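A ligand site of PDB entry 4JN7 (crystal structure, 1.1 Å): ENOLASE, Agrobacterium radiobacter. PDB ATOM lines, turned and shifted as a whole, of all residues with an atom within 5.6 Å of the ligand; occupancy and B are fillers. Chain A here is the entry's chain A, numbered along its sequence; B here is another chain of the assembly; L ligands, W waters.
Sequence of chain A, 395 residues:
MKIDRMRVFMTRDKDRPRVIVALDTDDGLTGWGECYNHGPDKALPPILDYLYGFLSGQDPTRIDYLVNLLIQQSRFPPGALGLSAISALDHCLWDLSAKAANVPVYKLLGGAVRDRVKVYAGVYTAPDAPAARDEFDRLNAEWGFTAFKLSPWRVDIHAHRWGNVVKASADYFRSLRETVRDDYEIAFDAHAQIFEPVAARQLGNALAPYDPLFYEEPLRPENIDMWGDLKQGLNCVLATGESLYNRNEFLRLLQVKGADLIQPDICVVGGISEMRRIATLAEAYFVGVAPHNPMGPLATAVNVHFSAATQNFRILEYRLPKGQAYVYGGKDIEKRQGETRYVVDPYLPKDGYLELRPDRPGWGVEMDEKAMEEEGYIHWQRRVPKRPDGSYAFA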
ATOM      1  N   ARG A  16      13.350  12.702   8.092  1.00  0.00           N
ATOM      2  CA  ARG A  16      14.613  12.007   7.846  1.00  0.00           C
ATOM      3  C   ARG A  16      14.333  10.558   7.528  1.00  0.00           C
ATOM      4  O   ARG A  16      13.468   9.946   8.158  1.00  0.00           O
ATOM      5  CB  ARG A  16      15.519  12.115   9.068  1.00  0.00           C
ATOM      6  CG  ARG A  16      16.004  13.538   9.295  1.00  0.00           C
ATOM      7  CD  ARG A  16      16.908  13.736  10.493  1.00  0.00           C
ATOM      8  NE  ARG A  16      18.224  13.111  10.324  1.00  0.00           N
ATOM      9  CZ  ARG A  16      19.284  13.395  11.066  1.00  0.00           C
ATOM     10  NH1 ARG A  16      19.215  14.291  12.032  1.00  0.00           N
ATOM     11  NH2 ARG A  16      20.438  12.774  10.849  1.00  0.00           N
ATOM     12  N   TYR A  36      21.664   4.727  12.190  1.00  0.00           N
ATOM     13  CA  TYR A  36      21.717   6.180  12.135  1.00  0.00           C
ATOM     14  C   TYR A  36      21.432   6.657  10.709  1.00  0.00           C
ATOM     15  O   TYR A  36      21.771   5.977   9.740  1.00  0.00           O
ATOM     16  CB  TYR A  36      23.093   6.715  12.556  1.00  0.00           C
ATOM     17  CG  TYR A  36      23.071   8.192  12.882  1.00  0.00           C
ATOM     18  CD1 TYR A  36      22.621   8.628  14.109  1.00  0.00           C
ATOM     19  CD2 TYR A  36      23.473   9.153  11.954  1.00  0.00           C
ATOM     20  CE1 TYR A  36      22.565   9.959  14.420  1.00  0.00           C
ATOM     21  CE2 TYR A  36      23.428  10.504  12.274  1.00  0.00           C
ATOM     22  CZ  TYR A  36      22.961  10.895  13.510  1.00  0.00           C
ATOM     23  OH  TYR A  36      22.896  12.216  13.864  1.00  0.00           O
ATOM     24  N   ASN A  37      20.833   7.837  10.575  1.00  0.00           N
ATOM     25  CA  ASN A  37      20.642   8.491   9.284  1.00  0.00           C
ATOM     26  C   ASN A  37      21.774   9.475   8.986  1.00  0.00           C
ATOM     27  O   ASN A  37      21.686  10.658   9.294  1.00  0.00           O
ATOM     28  CB  ASN A  37      19.278   9.209   9.247  1.00  0.00           C
ATOM     29  CG  ASN A  37      19.134  10.171   8.077  1.00  0.00           C
ATOM     30  OD1 ASN A  37      18.647  11.283   8.223  1.00  0.00           O
ATOM     31  ND2 ASN A  37      19.581   9.752   6.905  1.00  0.00           N
ATOM     32  N   TYR A 124      16.264  22.402  20.267  1.00  0.00           N
ATOM     33  CA  TYR A 124      17.260  22.619  19.211  1.00  0.00           C
ATOM     34  C   TYR A 124      17.275  24.000  18.582  1.00  0.00           C
ATOM     35  O   TYR A 124      18.180  24.310  17.830  1.00  0.00           O
ATOM     36  CB  TYR A 124      17.135  21.595  18.081  1.00  0.00           C
ATOM     37  CG  TYR A 124      17.206  20.149  18.503  1.00  0.00           C
ATOM     38  CD1 TYR A 124      18.318  19.626  19.155  1.00  0.00           C
ATOM     39  CD2 TYR A 124      16.182  19.281  18.199  1.00  0.00           C
ATOM     40  CE1 TYR A 124      18.386  18.281  19.517  1.00  0.00           C
ATOM     41  CE2 TYR A 124      16.238  17.948  18.537  1.00  0.00           C
ATOM     42  CZ  TYR A 124      17.345  17.444  19.201  1.00  0.00           C
ATOM     43  OH  TYR A 124      17.368  16.116  19.524  1.00  0.00           O
ATOM     44  N   ASP A 189      23.613  23.351  22.476  1.00  0.00           N
ATOM     45  CA  ASP A 189      24.338  22.609  21.445  1.00  0.00           C
ATOM     46  C   ASP A 189      24.860  23.578  20.406  1.00  0.00           C
ATOM     47  O   ASP A 189      24.094  24.161  19.645  1.00  0.00           O
ATOM     48  CB  ASP A 189      23.391  21.595  20.801  1.00  0.00           C
ATOM     49  CG  ASP A 189      24.091  20.655  19.845  1.00  0.00           C
ATOM     50  OD1 ASP A 189      25.253  20.916  19.472  1.00  0.00           O
ATOM     51  OD2 ASP A 189      23.433  19.651  19.490  1.00  0.00           O
ATOM     52  N   HIS A 191      26.800  22.806  17.989  1.00  0.00           N
ATOM     53  CA  HIS A 191      26.621  22.136  16.700  1.00  0.00           C
ATOM     54  C   HIS A 191      27.845  22.165  15.787  1.00  0.00           C
ATOM     55  O   HIS A 191      27.700  22.209  14.559  1.00  0.00           O
ATOM     56  CB  HIS A 191      25.392  22.674  15.965  1.00  0.00           C
ATOM     57  CG  HIS A 191      24.677  21.623  15.177  1.00  0.00           C
ATOM     58  ND1 HIS A 191      24.760  21.493  13.801  1.00  0.00           N
ATOM     59  CD2 HIS A 191      23.857  20.624  15.600  1.00  0.00           C
ATOM     60  CE1 HIS A 191      24.008  20.478  13.411  1.00  0.00           C
ATOM     61  NE2 HIS A 191      23.451  19.932  14.479  1.00  0.00           N
ATOM     62  N   GLU A 216      27.536  21.671  24.415  1.00  0.00           N
ATOM     63  CA  GLU A 216      27.744  20.537  23.526  1.00  0.00           C
ATOM     64  C   GLU A 216      28.401  20.880  22.211  1.00  0.00           C
ATOM     65  O   GLU A 216      28.034  21.824  21.488  1.00  0.00           O
ATOM     66  CB  GLU A 216      26.399  19.850  23.251  1.00  0.00           C
ATOM     67  CG  GLU A 216      26.412  18.860  22.086  1.00  0.00           C
ATOM     68  CD  GLU A 216      25.153  18.012  21.996  1.00  0.00           C
ATOM     69  OE1 GLU A 216      24.299  18.138  22.895  1.00  0.00           O
ATOM     70  OE2 GLU A 216      25.048  17.178  21.056  1.00  0.00           O
ATOM     71  N   GLU A 217      29.394  20.042  21.887  1.00  0.00           N
ATOM     72  CA  GLU A 217      30.047  19.954  20.587  1.00  0.00           C
ATOM     73  C   GLU A 217      30.362  21.299  19.926  1.00  0.00           C
ATOM     74  O   GLU A 217      29.989  21.527  18.783  1.00  0.00           O
ATOM     75  CB  GLU A 217      29.293  19.020  19.619  1.00  0.00           C
ATOM     76  CG  GLU A 217      30.231  18.463  18.539  1.00  0.00           C
ATOM     77  CD  GLU A 217      29.587  17.550  17.508  1.00  0.00           C
ATOM     78  OE1 GLU A 217      28.381  17.714  17.198  1.00  0.00           O
ATOM     79  OE2 GLU A 217      30.347  16.706  16.972  1.00  0.00           O
ATOM     80  N   GLU A 242      29.344  12.875  19.760  1.00  0.00           N
ATOM     81  CA  GLU A 242      28.430  12.250  18.807  1.00  0.00           C
ATOM     82  C   GLU A 242      29.108  11.882  17.510  1.00  0.00           C
ATOM     83  O   GLU A 242      28.664  10.952  16.825  1.00  0.00           O
ATOM     84  CB  GLU A 242      27.282  13.186  18.491  1.00  0.00           C
ATOM     85  CG  GLU A 242      27.665  14.425  17.721  1.00  0.00           C
ATOM     86  CD  GLU A 242      26.481  15.341  17.525  1.00  0.00           C
ATOM     87  OE1 GLU A 242      25.966  15.846  18.531  1.00  0.00           O
ATOM     88  OE2 GLU A 242      26.038  15.519  16.357  1.00  0.00           O
ATOM     89  N   HIS A 292      23.965  10.556  22.668  1.00  0.00           N
ATOM     90  CA  HIS A 292      23.392  11.314  21.551  1.00  0.00           C
ATOM     91  C   HIS A 292      22.244  10.517  20.963  1.00  0.00           C
ATOM     92  O   HIS A 292      22.368   9.326  20.683  1.00  0.00           O
ATOM     93  CB  HIS A 292      24.482  11.507  20.515  1.00  0.00           C
ATOM     94  CG  HIS A 292      24.067  12.263  19.284  1.00  0.00           C
ATOM     95  ND1 HIS A 292      23.866  11.643  18.069  1.00  0.00           N
ATOM     96  CD2 HIS A 292      23.876  13.594  19.084  1.00  0.00           C
ATOM     97  CE1 HIS A 292      23.579  12.574  17.165  1.00  0.00           C
ATOM     98  NE2 HIS A 292      23.570  13.759  17.752  1.00  0.00           N
ATOM     99  N   PRO A 294      19.152  11.903  18.485  1.00  0.00           N
ATOM    100  CA  PRO A 294      18.130  12.566  17.660  1.00  0.00           C
ATOM    101  C   PRO A 294      17.409  11.572  16.745  1.00  0.00           C
ATOM    102  O   PRO A 294      16.714  11.979  15.815  1.00  0.00           O
ATOM    103  CB  PRO A 294      18.954  13.535  16.824  1.00  0.00           C
ATOM    104  CG  PRO A 294      20.222  12.768  16.562  1.00  0.00           C
ATOM    105  CD  PRO A 294      20.492  12.011  17.867  1.00  0.00           C
ATOM    106  N   MET A 295      17.605  10.281  16.997  1.00  0.00           N
ATOM    107  CA  MET A 295      17.033   9.213  16.177  1.00  0.00           C
ATOM    108  C   MET A 295      15.638   8.840  16.722  1.00  0.00           C
ATOM    109  O   MET A 295      15.025   9.596  17.496  1.00  0.00           O
ATOM    110  CB  MET A 295      18.013   8.036  16.072  1.00  0.00           C
ATOM    111  CG  MET A 295      19.280   8.388  15.261  1.00  0.00           C
ATOM    112  SD  MET A 295      18.933   8.732  13.511  1.00  0.00           S
ATOM    113  CE  MET A 295      19.079  10.522  13.456  1.00  0.00           C
ATOM    114  N   GLU A 317      19.158  12.180  25.522  1.00  0.00           N
ATOM    115  CA  GLU A 317      18.508  13.021  24.518  1.00  0.00           C
ATOM    116  C   GLU A 317      17.231  12.346  24.004  1.00  0.00           C
ATOM    117  O   GLU A 317      17.237  11.151  23.725  1.00  0.00           O
ATOM    118  CB  GLU A 317      19.472  13.227  23.349  1.00  0.00           C
ATOM    119  CG  GLU A 317      18.940  14.168  22.268  1.00  0.00           C
ATOM    120  CD  GLU A 317      20.003  14.580  21.276  1.00  0.00           C
ATOM    121  OE1 GLU A 317      21.109  13.978  21.265  1.00  0.00           O
ATOM    122  OE2 GLU A 317      19.754  15.548  20.541  1.00  0.00           O
ATOM    123  N   TYR A 326      12.752  17.422  12.332  1.00  0.00           N
ATOM    124  CA  TYR A 326      14.144  17.726  12.605  1.00  0.00           C
ATOM    125  C   TYR A 326      14.472  19.188  12.312  1.00  0.00           C
ATOM    126  O   TYR A 326      14.070  19.737  11.300  1.00  0.00           O
ATOM    127  CB  TYR A 326      15.122  16.814  11.834  1.00  0.00           C
ATOM    128  CG  TYR A 326      16.530  17.254  12.147  1.00  0.00           C
ATOM    129  CD1 TYR A 326      17.163  16.842  13.310  1.00  0.00           C
ATOM    130  CD2 TYR A 326      17.192  18.153  11.316  1.00  0.00           C
ATOM    131  CE1 TYR A 326      18.434  17.289  13.623  1.00  0.00           C
ATOM    132  CE2 TYR A 326      18.470  18.592  11.626  1.00  0.00           C
ATOM    133  CZ  TYR A 326      19.084  18.157  12.773  1.00  0.00           C
ATOM    134  OH  TYR A 326      20.347  18.615  13.076  1.00  0.00           O
ATOM    135  N   TRP A 380      16.984  13.608   2.594  1.00  0.00           N
ATOM    136  CA  TRP A 380      17.318  14.579   3.611  1.00  0.00           C
ATOM    137  C   TRP A 380      18.785  14.936   3.483  1.00  0.00           C
ATOM    138  O   TRP A 380      19.621  14.055   3.248  1.00  0.00           O
ATOM    139  CB  TRP A 380      17.039  14.022   5.002  1.00  0.00           C
ATOM    140  CG  TRP A 380      17.426  14.934   6.145  1.00  0.00           C
ATOM    141  CD1 TRP A 380      16.668  15.930   6.682  1.00  0.00           C
ATOM    142  CD2 TRP A 380      18.657  14.929   6.880  1.00  0.00           C
ATOM    143  NE1 TRP A 380      17.348  16.548   7.711  1.00  0.00           N
ATOM    144  CE2 TRP A 380      18.575  15.950   7.845  1.00  0.00           C
ATOM    145  CE3 TRP A 380      19.829  14.161   6.806  1.00  0.00           C
ATOM    146  CZ2 TRP A 380      19.616  16.217   8.735  1.00  0.00           C
ATOM    147  CZ3 TRP A 380      20.851  14.439   7.694  1.00  0.00           C
ATOM    148  CH2 TRP A 380      20.739  15.452   8.649  1.00  0.00           C
ATOM    149  N   ARG A 382      21.912  17.956   5.073  1.00  0.00           N
ATOM    150  CA  ARG A 382      22.293  19.020   5.982  1.00  0.00           C
ATOM    151  C   ARG A 382      22.430  20.333   5.263  1.00  0.00           C
ATOM    152  O   ARG A 382      22.633  20.384   4.069  1.00  0.00           O
ATOM    153  CB  ARG A 382      23.624  18.689   6.652  1.00  0.00           C
ATOM    154  CG  ARG A 382      23.557  17.462   7.515  1.00  0.00           C
ATOM    155  CD  ARG A 382      24.874  17.070   8.168  1.00  0.00           C
ATOM    156  NE  ARG A 382      24.627  15.856   8.923  1.00  0.00           N
ATOM    157  CZ  ARG A 382      24.565  14.635   8.380  1.00  0.00           C
ATOM    158  NH1 ARG A 382      24.867  14.436   7.099  1.00  0.00           N
ATOM    159  NH2 ARG A 382      24.203  13.621   9.141  1.00  0.00           N
ATOM    160  N   ARG B  75      29.421  15.873   7.451  1.00  0.00           N
ATOM    161  CA  ARG B  75      29.555  16.423   8.812  1.00  0.00           C
ATOM    162  C   ARG B  75      30.312  15.485   9.737  1.00  0.00           C
ATOM    163  O   ARG B  75      31.321  15.880  10.358  1.00  0.00           O
ATOM    164  CB  ARG B  75      28.213  16.797   9.442  1.00  0.00           C
ATOM    165  CG  ARG B  75      28.364  17.609  10.722  1.00  0.00           C
ATOM    166  CD  ARG B  75      27.027  17.805  11.403  1.00  0.00           C
ATOM    167  NE  ARG B  75      27.084  18.734  12.526  1.00  0.00           N
ATOM    168  CZ  ARG B  75      27.193  18.394  13.811  1.00  0.00           C
ATOM    169  NH1 ARG B  75      27.307  17.125  14.179  1.00  0.00           N
ATOM    170  NH2 ARG B  75      27.186  19.327  14.742  1.00  0.00           N
ATOM    171  N   PHE B  76      29.816  14.251   9.883  1.00  0.00           N
ATOM    172  CA  PHE B  76      30.558  13.203  10.561  1.00  0.00           C
ATOM    173  C   PHE B  76      31.766  12.880   9.681  1.00  0.00           C
ATOM    174  O   PHE B  76      31.651  12.825   8.456  1.00  0.00           O
ATOM    175  CB  PHE B  76      29.696  11.949  10.666  1.00  0.00           C
ATOM    176  CG  PHE B  76      28.542  12.058  11.623  1.00  0.00           C
ATOM    177  CD1 PHE B  76      27.339  12.665  11.265  1.00  0.00           C
ATOM    178  CD2 PHE B  76      28.664  11.529  12.895  1.00  0.00           C
ATOM    179  CE1 PHE B  76      26.306  12.761  12.165  1.00  0.00           C
ATOM    180  CE2 PHE B  76      27.623  11.614  13.809  1.00  0.00           C
ATOM    181  CZ  PHE B  76      26.421  12.239  13.440  1.00  0.00           C
HETATM  182  C1  LIG L   1      23.040  15.248  12.212  1.00  0.00           C
HETATM  183  O1  LIG L   1      23.573  16.115  11.466  1.00  0.00           O
HETATM  184  O2  LIG L   1      22.944  14.038  11.818  1.00  0.00           O
HETATM  185  C2  LIG L   1      22.348  15.781  13.398  1.00  0.00           C
HETATM  186  O3  LIG L   1      21.349  14.938  13.838  1.00  0.00           O
HETATM  187  C3  LIG L   1      23.431  15.903  14.404  1.00  0.00           C
HETATM  188  C4  LIG L   1      22.960  16.573  15.648  1.00  0.00           C
HETATM  189  O4  LIG L   1      23.669  16.535  16.674  1.00  0.00           O
HETATM  190  O5  LIG L   1      21.871  17.210  15.714  1.00  0.00           O
HETATM  191  O   HOH W   1      25.962  18.873  17.784  1.00  0.00           O
HETATM  192  O   HOH W   2      22.669  18.698  11.259  1.00  0.00           O
HETATM  193  O   HOH W   3      21.973  16.501  19.213  1.00  0.00           O
HETATM  194  O   HOH W   4      19.609  19.547  15.908  1.00  0.00           O
HETATM  195  O   HOH W   5      21.349  18.834  17.667  1.00  0.00           O
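Water W5 bridges O5 of the ligand (2.6 Å) and OD2 of Asp 189 (2.9 Å). Water W2 bridges O1 of the ligand and OH of Tyr 326. Water W3 lies within hydrogen-bond range of the side-chain carboxylate (OE2) of Glu 317 (2.8 Å), an oxygen (O4) of the ligand (3.1 Å), the side-chain carboxylate (OD2) of Asp 189 (3.5 Å) and a ring nitrogen (NE2) of His 292 (3.5 Å). Water W4 bridges the side-chain hydroxyl of Tyr 326 (3.1 Å) and an oxygen (O5) of the ligand (3.3 Å).
OE1 of Glu 242 lies close to NE2 of His 292 (3.3 Å). The guanidinium group of Arg 75 of chain B is in salt-bridge range of the side-chain carboxylate of Glu 217 (3.2 Å). The guanidinium group (NH2) of Arg 75 of chain B is in hydrogen-bond range of the backbone carbonyl oxygen (O) of His 191 (2.9 Å). OE2 of Glu 242 lies within salt-bridge range of NH1 of Arg 75 of chain B (3.0 Å). N of His 191 lies within hydrogen-bond range of OD1 of Asp 189, 2.9 Å away. NE of Arg 16 sits at hydrogen-bond distance from OD1 of Asn 37 (2.8 Å).
Residues that only touch the ligand: Phe 76 of chain B, Pro 294 and Arg 75 of chain B. Hydrophobic or aromatic side chains within 4 Å of the ligand: Tyr 36, His 191, His 292, Pro 294, Tyr 326 and Phe 76 of chain B. Along chain A the residues within 4 Å of the ligand span positions 16 to 382. The nearest printed residue that does not touch the ligand is Trp 380 (4.1 Å).
An oxygen (O5) of the ligand is in hydrogen-bond range of a ring nitrogen (NE2) of His 191. O5 of the ligand sits at hydrogen-bond distance from OH of Tyr 326 (3.4 Å). NH2 of Arg 16 is in salt-bridge range of O2 of the ligand (3.0 Å). NE of Arg 382 lies within salt-bridge range of O1 of the ligand (2.8 Å). The side-chain hydroxyl (OH) of Tyr 36 sits at hydrogen-bond distance from an oxygen (O2) of the ligand, 2.7 Å away. A ring nitrogen (NE2) of His 292 is in hydrogen-bond range of an oxygen (O4) of the ligand (3.0 Å). O4 of the ligand sits close to OE2 of Glu 242 (2.6 Å).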
